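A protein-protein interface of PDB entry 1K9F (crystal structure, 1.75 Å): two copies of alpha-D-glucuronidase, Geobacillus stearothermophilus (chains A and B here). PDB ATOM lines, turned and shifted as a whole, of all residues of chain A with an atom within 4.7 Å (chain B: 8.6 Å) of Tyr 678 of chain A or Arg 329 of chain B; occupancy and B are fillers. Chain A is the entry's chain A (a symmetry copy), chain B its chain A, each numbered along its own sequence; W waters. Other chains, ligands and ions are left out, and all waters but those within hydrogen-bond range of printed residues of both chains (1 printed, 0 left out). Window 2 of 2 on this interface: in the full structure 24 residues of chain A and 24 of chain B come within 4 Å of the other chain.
No position is printed for both chains. Of the 10 pairs that touch across the chains among the printed residues, none has its exchanged pair printed and touching as well.
Water W1 bridges OE2 of Glu 654 of chain A (2.7 Å) and O of Tyr 537 of chain B (2.8 Å).
Hydrophobic or aromatic side chains of chain A within 4 Å of the printed part of chain B: Tyr 678. Among the printed residues, Asp or Glu carboxylates within 4 Å of a Lys or Arg side-chain nitrogen of the other chain: Glu 654 of chain A with Arg 329 of chain B (2.9 Å) and Asp 657 of chain A with Arg 329 of chain B (2.9 Å).
Among the printed residues, pairs that only touch across the chains: Thr 661 of chain A with Trp 328 of chain B (3.4 Å), Tyr 678 of chain A with Arg 329 of chain B (3.5 Å), Asp 657 of chain A with Trp 328 of chain B (3.6 Å), Lys 653 of chain A with Arg 329 of chain B (3.6 Å) and Thr 661 of chain A with Tyr 537 of chain B (3.9 Å).
Printed residues of chain B within 4 Å of Lys 653 of chain A: Arg 329. Of the printed residues of chain B, Tyr 678 of chain A touches Arg 329 (3.5 Å). Of the printed residues of chain A, Arg 329 of chain B touches Lys 653, Glu 654, Asp 657, Tyr 678 and Arg 679. Of the printed residues of chain A, Arg 331 of chain B touches Arg 679 (2.9 Å). Thr 333 of chain B touches none of the printed residues of chain A.
The side-chain carboxylate (OD1) of Asp 327 of chain B lies within salt-bridge range of the guanidinium group (NH1) of Arg 329 of chain B, 2.8 Å away. The side-chain hydroxyl (OG1) of Thr 661 of chain A is in hydrogen-bond range of the backbone carbonyl oxygen (O) of Asp 657 of chain A (3.1 Å). OG1 of Thr 661 of chain A sits at hydrogen-bond distance from O of Tyr 678 of chain A, at 2.7 Å.
The backbone carbonyl oxygen (O) of Arg 329 of chain B is in hydrogen-bond range of the guanidinium group (NH1) of Arg 679 of chain A. The guanidinium group of Arg 331 of chain B is in salt-bridge range of the chain-end carboxylate of Arg 679 of chain A, at 2.9 Å. The indole nitrogen (NE1) of Trp 328 of chain B lies within hydrogen-bond range of the side-chain carboxylate (OE2) of Glu 654 of chain A (2.9 Å). OE1 of Glu 654 of chain A lies within salt-bridge range of NH2 of Arg 329 of chain B, at 2.9 Å. The guanidinium group (NE) of Arg 329 of chain B lies within salt-bridge range of the side-chain carboxylate (OD2) of Asp 657 of chain A (2.9 Å).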
ATOM      1  N   LYS A 653       7.864   8.330 -30.715  1.00  0.00           N
ATOM      2  CA  LYS A 653       8.030   6.928 -30.346  1.00  0.00           C
ATOM      3  C   LYS A 653       6.666   6.297 -30.068  1.00  0.00           C
ATOM      4  O   LYS A 653       6.436   5.125 -30.370  1.00  0.00           O
ATOM      5  CB  LYS A 653       8.908   6.804 -29.095  1.00  0.00           C
ATOM      6  CG  LYS A 653      10.384   7.086 -29.331  1.00  0.00           C
ATOM      7  CD  LYS A 653      11.137   7.154 -28.010  1.00  0.00           C
ATOM      8  CE  LYS A 653      12.602   7.509 -28.225  1.00  0.00           C
ATOM      9  NZ  LYS A 653      13.331   7.661 -26.930  1.00  0.00           N
ATOM     10  N   GLU A 654       5.764   7.080 -29.484  1.00  0.00           N
ATOM     11  CA  GLU A 654       4.423   6.598 -29.170  1.00  0.00           C
ATOM     12  C   GLU A 654       3.655   6.395 -30.479  1.00  0.00           C
ATOM     13  O   GLU A 654       2.986   5.378 -30.661  1.00  0.00           O
ATOM     14  CB  GLU A 654       3.702   7.611 -28.274  1.00  0.00           C
ATOM     15  CG  GLU A 654       2.376   7.128 -27.695  1.00  0.00           C
ATOM     16  CD  GLU A 654       2.531   5.996 -26.691  1.00  0.00           C
ATOM     17  OE1 GLU A 654       3.666   5.738 -26.228  1.00  0.00           O
ATOM     18  OE2 GLU A 654       1.502   5.369 -26.355  1.00  0.00           O
ATOM     19  N   ASP A 657       5.096   3.170 -32.256  1.00  0.00           N
ATOM     20  CA  ASP A 657       4.691   1.908 -31.667  1.00  0.00           C
ATOM     21  C   ASP A 657       3.192   1.634 -31.710  1.00  0.00           C
ATOM     22  O   ASP A 657       2.783   0.512 -31.988  1.00  0.00           O
ATOM     23  CB  ASP A 657       5.221   1.799 -30.231  1.00  0.00           C
ATOM     24  CG  ASP A 657       6.750   1.800 -30.170  1.00  0.00           C
ATOM     25  OD1 ASP A 657       7.400   1.433 -31.179  1.00  0.00           O
ATOM     26  OD2 ASP A 657       7.304   2.154 -29.107  1.00  0.00           O
ATOM     27  N   THR A 661       2.024  -1.539 -33.845  1.00  0.00           N
ATOM     28  CA  THR A 661       1.356  -2.620 -33.126  1.00  0.00           C
ATOM     29  C   THR A 661      -0.063  -2.832 -33.640  1.00  0.00           C
ATOM     30  O   THR A 661      -0.502  -3.967 -33.825  1.00  0.00           O
ATOM     31  CB  THR A 661       1.315  -2.347 -31.610  1.00  0.00           C
ATOM     32  OG1 THR A 661       2.648  -2.410 -31.084  1.00  0.00           O
ATOM     33  CG2 THR A 661       0.438  -3.382 -30.896  1.00  0.00           C
ATOM     34  N   LYS A 676      11.718  -3.699 -33.421  1.00  0.00           N
ATOM     35  CA  LYS A 676      10.811  -3.905 -32.304  1.00  0.00           C
ATOM     36  C   LYS A 676       9.367  -3.439 -32.438  1.00  0.00           C
ATOM     37  O   LYS A 676       9.086  -2.244 -32.494  1.00  0.00           O
ATOM     38  CB  LYS A 676      11.417  -3.303 -31.030  1.00  0.00           C
ATOM     39  CG  LYS A 676      10.644  -3.632 -29.754  1.00  0.00           C
ATOM     40  CD  LYS A 676      10.604  -5.134 -29.501  1.00  0.00           C
ATOM     41  CE  LYS A 676       9.813  -5.470 -28.247  1.00  0.00           C
ATOM     42  NZ  LYS A 676       9.717  -6.945 -28.030  1.00  0.00           N
ATOM     43  N   ILE A 677       8.461  -4.407 -32.500  1.00  0.00           N
ATOM     44  CA  ILE A 677       7.032  -4.123 -32.551  1.00  0.00           C
ATOM     45  C   ILE A 677       6.468  -4.828 -31.321  1.00  0.00           C
ATOM     46  O   ILE A 677       6.634  -6.038 -31.158  1.00  0.00           O
ATOM     47  CB  ILE A 677       6.348  -4.696 -33.809  1.00  0.00           C
ATOM     48  CG1 ILE A 677       6.858  -3.974 -35.060  1.00  0.00           C
ATOM     49  CG2 ILE A 677       4.823  -4.529 -33.694  1.00  0.00           C
ATOM     50  CD1 ILE A 677       6.204  -4.451 -36.352  1.00  0.00           C
ATOM     51  N   TYR A 678       5.829  -4.071 -30.439  1.00  0.00           N
ATOM     52  CA  TYR A 678       5.266  -4.667 -29.242  1.00  0.00           C
ATOM     53  C   TYR A 678       3.998  -5.445 -29.583  1.00  0.00           C
ATOM     54  O   TYR A 678       3.064  -4.910 -30.177  1.00  0.00           O
ATOM     55  CB  TYR A 678       5.005  -3.579 -28.193  1.00  0.00           C
ATOM     56  CG  TYR A 678       6.281  -2.883 -27.760  1.00  0.00           C
ATOM     57  CD1 TYR A 678       6.781  -1.788 -28.468  1.00  0.00           C
ATOM     58  CD2 TYR A 678       7.027  -3.366 -26.686  1.00  0.00           C
ATOM     59  CE1 TYR A 678       7.992  -1.196 -28.119  1.00  0.00           C
ATOM     60  CE2 TYR A 678       8.240  -2.783 -26.331  1.00  0.00           C
ATOM     61  CZ  TYR A 678       8.717  -1.702 -27.051  1.00  0.00           C
ATOM     62  OH  TYR A 678       9.924  -1.138 -26.711  1.00  0.00           O
ATOM     63  N   ARG A 679       4.000  -6.723 -29.211  1.00  0.00           N
ATOM     64  CA  ARG A 679       2.898  -7.655 -29.458  1.00  0.00           C
ATOM     65  C   ARG A 679       1.494  -7.112 -29.184  1.00  0.00           C
ATOM     66  O   ARG A 679       0.604  -7.341 -30.034  1.00  0.00           O
ATOM     67  CB  ARG A 679       3.112  -8.933 -28.636  1.00  0.00           C
ATOM     68  CG  ARG A 679       2.738  -8.821 -27.155  1.00  0.00           C
ATOM     69  CD  ARG A 679       3.451  -7.674 -26.455  1.00  0.00           C
ATOM     70  NE  ARG A 679       4.903  -7.787 -26.549  1.00  0.00           N
ATOM     71  CZ  ARG A 679       5.755  -6.913 -26.022  1.00  0.00           C
ATOM     72  NH1 ARG A 679       5.300  -5.858 -25.359  1.00  0.00           N
ATOM     73  NH2 ARG A 679       7.063  -7.093 -26.162  1.00  0.00           N
ATOM     74  OXT ARG A 679       1.287  -6.494 -28.117  1.00  0.00           O
ATOM     75  N   GLN B 326       0.406   3.850 -16.847  1.00  0.00           N
ATOM     76  CA  GLN B 326       0.948   2.565 -17.259  1.00  0.00           C
ATOM     77  C   GLN B 326       1.267   2.531 -18.754  1.00  0.00           C
ATOM     78  O   GLN B 326       0.593   3.172 -19.559  1.00  0.00           O
ATOM     79  CB  GLN B 326      -0.046   1.452 -16.917  1.00  0.00           C
ATOM     80  CG  GLN B 326       0.439   0.057 -17.265  1.00  0.00           C
ATOM     81  CD  GLN B 326      -0.573  -1.021 -16.919  1.00  0.00           C
ATOM     82  OE1 GLN B 326      -0.470  -2.155 -17.385  1.00  0.00           O
ATOM     83  NE2 GLN B 326      -1.555  -0.673 -16.092  1.00  0.00           N
ATOM     84  N   ASP B 327       2.304   1.786 -19.117  1.00  0.00           N
ATOM     85  CA  ASP B 327       2.693   1.665 -20.518  1.00  0.00           C
ATOM     86  C   ASP B 327       1.944   0.472 -21.109  1.00  0.00           C
ATOM     87  O   ASP B 327       2.068  -0.649 -20.618  1.00  0.00           O
ATOM     88  CB  ASP B 327       4.201   1.437 -20.635  1.00  0.00           C
ATOM     89  CG  ASP B 327       4.704   1.603 -22.054  1.00  0.00           C
ATOM     90  OD1 ASP B 327       3.938   1.308 -22.992  1.00  0.00           O
ATOM     91  OD2 ASP B 327       5.869   2.019 -22.231  1.00  0.00           O
ATOM     92  N   TRP B 328       1.168   0.706 -22.162  1.00  0.00           N
ATOM     93  CA  TRP B 328       0.410  -0.380 -22.778  1.00  0.00           C
ATOM     94  C   TRP B 328       1.305  -1.488 -23.333  1.00  0.00           C
ATOM     95  O   TRP B 328       0.851  -2.614 -23.542  1.00  0.00           O
ATOM     96  CB  TRP B 328      -0.500   0.158 -23.895  1.00  0.00           C
ATOM     97  CG  TRP B 328       0.217   0.884 -24.989  1.00  0.00           C
ATOM     98  CD1 TRP B 328       0.448   2.225 -25.072  1.00  0.00           C
ATOM     99  CD2 TRP B 328       0.827   0.299 -26.148  1.00  0.00           C
ATOM    100  NE1 TRP B 328       1.162   2.516 -26.211  1.00  0.00           N
ATOM    101  CE2 TRP B 328       1.409   1.351 -26.889  1.00  0.00           C
ATOM    102  CE3 TRP B 328       0.938  -1.011 -26.630  1.00  0.00           C
ATOM    103  CZ2 TRP B 328       2.097   1.131 -28.091  1.00  0.00           C
ATOM    104  CZ3 TRP B 328       1.624  -1.231 -27.827  1.00  0.00           C
ATOM    105  CH2 TRP B 328       2.191  -0.163 -28.542  1.00  0.00           C
ATOM    106  N   ARG B 329       2.574  -1.164 -23.570  1.00  0.00           N
ATOM    107  CA  ARG B 329       3.535  -2.126 -24.109  1.00  0.00           C
ATOM    108  C   ARG B 329       3.930  -3.187 -23.087  1.00  0.00           C
ATOM    109  O   ARG B 329       4.191  -4.336 -23.435  1.00  0.00           O
ATOM    110  CB  ARG B 329       4.814  -1.414 -24.544  1.00  0.00           C
ATOM    111  CG  ARG B 329       4.643  -0.257 -25.509  1.00  0.00           C
ATOM    112  CD  ARG B 329       6.005   0.386 -25.724  1.00  0.00           C
ATOM    113  NE  ARG B 329       5.989   1.534 -26.626  1.00  0.00           N
ATOM    114  CZ  ARG B 329       5.412   2.701 -26.358  1.00  0.00           C
ATOM    115  NH1 ARG B 329       4.783   2.890 -25.205  1.00  0.00           N
ATOM    116  NH2 ARG B 329       5.495   3.690 -27.236  1.00  0.00           N
ATOM    117  N   ASP B 330       3.986  -2.776 -21.826  1.00  0.00           N
ATOM    118  CA  ASP B 330       4.388  -3.651 -20.732  1.00  0.00           C
ATOM    119  C   ASP B 330       3.276  -4.581 -20.252  1.00  0.00           C
ATOM    120  O   ASP B 330       2.414  -4.176 -19.473  1.00  0.00           O
ATOM    121  CB  ASP B 330       4.899  -2.780 -19.584  1.00  0.00           C
ATOM    122  CG  ASP B 330       5.367  -3.588 -18.396  1.00  0.00           C
ATOM    123  OD1 ASP B 330       5.892  -4.702 -18.601  1.00  0.00           O
ATOM    124  OD2 ASP B 330       5.221  -3.093 -17.260  1.00  0.00           O
ATOM    125  N   ARG B 331       3.303  -5.827 -20.717  1.00  0.00           N
ATOM    126  CA  ARG B 331       2.291  -6.805 -20.335  1.00  0.00           C
ATOM    127  C   ARG B 331       2.588  -7.497 -19.008  1.00  0.00           C
ATOM    128  O   ARG B 331       1.892  -8.440 -18.632  1.00  0.00           O
ATOM    129  CB  ARG B 331       2.111  -7.869 -21.427  1.00  0.00           C
ATOM    130  CG  ARG B 331       1.483  -7.359 -22.724  1.00  0.00           C
ATOM    131  CD  ARG B 331       0.851  -8.503 -23.521  1.00  0.00           C
ATOM    132  NE  ARG B 331       0.438  -8.081 -24.859  1.00  0.00           N
ATOM    133  CZ  ARG B 331      -0.278  -8.826 -25.697  1.00  0.00           C
ATOM    134  NH1 ARG B 331      -0.677 -10.041 -25.343  1.00  0.00           N
ATOM    135  NH2 ARG B 331      -0.591  -8.360 -26.900  1.00  0.00           N
ATOM    136  N   THR B 332       3.616  -7.036 -18.300  1.00  0.00           N
ATOM    137  CA  THR B 332       3.948  -7.623 -17.006  1.00  0.00           C
ATOM    138  C   THR B 332       3.254  -6.819 -15.908  1.00  0.00           C
ATOM    139  O   THR B 332       3.032  -7.320 -14.806  1.00  0.00           O
ATOM    140  CB  THR B 332       5.471  -7.631 -16.740  1.00  0.00           C
ATOM    141  OG1 THR B 332       5.953  -6.288 -16.635  1.00  0.00           O
ATOM    142  CG2 THR B 332       6.203  -8.345 -17.865  1.00  0.00           C
ATOM    143  N   THR B 333       2.919  -5.567 -16.212  1.00  0.00           N
ATOM    144  CA  THR B 333       2.229  -4.713 -15.252  1.00  0.00           C
ATOM    145  C   THR B 333       0.727  -4.917 -15.444  1.00  0.00           C
ATOM    146  O   THR B 333       0.225  -4.869 -16.568  1.00  0.00           O
ATOM    147  CB  THR B 333       2.581  -3.223 -15.458  1.00  0.00           C
ATOM    148  OG1 THR B 333       3.957  -3.007 -15.121  1.00  0.00           O
ATOM    149  CG2 THR B 333       1.711  -2.341 -14.574  1.00  0.00           C
ATOM    150  N   GLU B 536      -7.529   1.188 -25.627  1.00  0.00           N
ATOM    151  CA  GLU B 536      -6.606   0.096 -25.946  1.00  0.00           C
ATOM    152  C   GLU B 536      -5.118   0.452 -26.026  1.00  0.00           C
ATOM    153  O   GLU B 536      -4.270  -0.410 -25.799  1.00  0.00           O
ATOM    154  CB  GLU B 536      -7.068  -0.602 -27.237  1.00  0.00           C
ATOM    155  CG  GLU B 536      -6.338  -1.901 -27.581  1.00  0.00           C
ATOM    156  CD  GLU B 536      -6.459  -2.982 -26.510  1.00  0.00           C
ATOM    157  OE1 GLU B 536      -7.300  -2.849 -25.593  1.00  0.00           O
ATOM    158  OE2 GLU B 536      -5.708  -3.979 -26.597  1.00  0.00           O
ATOM    159  N   TYR B 537      -4.794   1.701 -26.347  1.00  0.00           N
ATOM    160  CA  TYR B 537      -3.392   2.117 -26.400  1.00  0.00           C
ATOM    161  C   TYR B 537      -3.154   3.291 -25.460  1.00  0.00           C
ATOM    162  O   TYR B 537      -2.223   4.081 -25.640  1.00  0.00           O
ATOM    163  CB  TYR B 537      -2.990   2.482 -27.832  1.00  0.00           C
ATOM    164  CG  TYR B 537      -3.103   1.311 -28.780  1.00  0.00           C
ATOM    165  CD1 TYR B 537      -4.315   1.005 -29.397  1.00  0.00           C
ATOM    166  CD2 TYR B 537      -2.010   0.474 -29.020  1.00  0.00           C
ATOM    167  CE1 TYR B 537      -4.440  -0.108 -30.230  1.00  0.00           C
ATOM    168  CE2 TYR B 537      -2.126  -0.642 -29.850  1.00  0.00           C
ATOM    169  CZ  TYR B 537      -3.343  -0.928 -30.450  1.00  0.00           C
ATOM    170  OH  TYR B 537      -3.472  -2.040 -31.253  1.00  0.00           O
ATOM    171  N   SER B 538      -4.005   3.396 -24.444  1.00  0.00           N
ATOM    172  CA  SER B 538      -3.896   4.474 -23.471  1.00  0.00           C
ATOM    173  C   SER B 538      -2.969   4.072 -22.338  1.00  0.00           C
ATOM    174  O   SER B 538      -2.425   2.967 -22.324  1.00  0.00           O
ATOM    175  CB  SER B 538      -5.268   4.809 -22.889  1.00  0.00           C
ATOM    176  OG  SER B 538      -5.723   3.746 -22.069  1.00  0.00           O
ATOM    177  N   HIS B 539      -2.815   4.977 -21.381  1.00  0.00           N
ATOM    178  CA  HIS B 539      -1.959   4.764 -20.223  1.00  0.00           C
ATOM    179  C   HIS B 539      -2.778   4.378 -18.990  1.00  0.00           C
ATOM    180  O   HIS B 539      -2.286   4.478 -17.863  1.00  0.00           O
ATOM    181  CB  HIS B 539      -1.179   6.049 -19.924  1.00  0.00           C
ATOM    182  CG  HIS B 539      -2.055   7.220 -19.591  1.00  0.00           C
ATOM    183  ND1 HIS B 539      -2.762   7.308 -18.411  1.00  0.00           N
ATOM    184  CD2 HIS B 539      -2.360   8.336 -20.295  1.00  0.00           C
ATOM    185  CE1 HIS B 539      -3.466   8.426 -18.403  1.00  0.00           C
ATOM    186  NE2 HIS B 539      -3.240   9.069 -19.534  1.00  0.00           N
ATOM    187  N   TYR B 543      -6.760  -2.879 -21.084  1.00  0.00           N
ATOM    188  CA  TYR B 543      -6.585  -3.461 -22.412  1.00  0.00           C
ATOM    189  C   TYR B 543      -7.241  -4.826 -22.603  1.00  0.00           C
ATOM    190  O   TYR B 543      -7.384  -5.590 -21.650  1.00  0.00           O
ATOM    191  CB  TYR B 543      -5.085  -3.599 -22.696  1.00  0.00           C
ATOM    192  CG  TYR B 543      -4.259  -2.441 -22.178  1.00  0.00           C
ATOM    193  CD1 TYR B 543      -4.460  -1.152 -22.660  1.00  0.00           C
ATOM    194  CD2 TYR B 543      -3.302  -2.630 -21.180  1.00  0.00           C
ATOM    195  CE1 TYR B 543      -3.730  -0.070 -22.163  1.00  0.00           C
ATOM    196  CE2 TYR B 543      -2.564  -1.555 -20.674  1.00  0.00           C
ATOM    197  CZ  TYR B 543      -2.786  -0.278 -21.171  1.00  0.00           C
ATOM    198  OH  TYR B 543      -2.078   0.796 -20.671  1.00  0.00           O
ATOM    199  N   TYR B 545      -6.282  -6.583 -25.639  1.00  0.00           N
ATOM    200  CA  TYR B 545      -5.280  -7.234 -26.491  1.00  0.00           C
ATOM    201  C   TYR B 545      -5.826  -7.997 -27.694  1.00  0.00           C
ATOM    202  O   TYR B 545      -5.225  -8.975 -28.148  1.00  0.00           O
ATOM    203  CB  TYR B 545      -4.424  -8.186 -25.655  1.00  0.00           C
ATOM    204  CG  TYR B 545      -3.724  -7.523 -24.491  1.00  0.00           C
ATOM    205  CD1 TYR B 545      -2.735  -6.563 -24.695  1.00  0.00           C
ATOM    206  CD2 TYR B 545      -4.057  -7.857 -23.182  1.00  0.00           C
ATOM    207  CE1 TYR B 545      -2.091  -5.952 -23.613  1.00  0.00           C
ATOM    208  CE2 TYR B 545      -3.427  -7.255 -22.102  1.00  0.00           C
ATOM    209  CZ  TYR B 545      -2.448  -6.309 -22.321  1.00  0.00           C
ATOM    210  OH  TYR B 545      -1.833  -5.730 -21.236  1.00  0.00           O
HETATM  211  O   HOH W   1      -1.007   6.371 -26.649  1.00  0.00           O
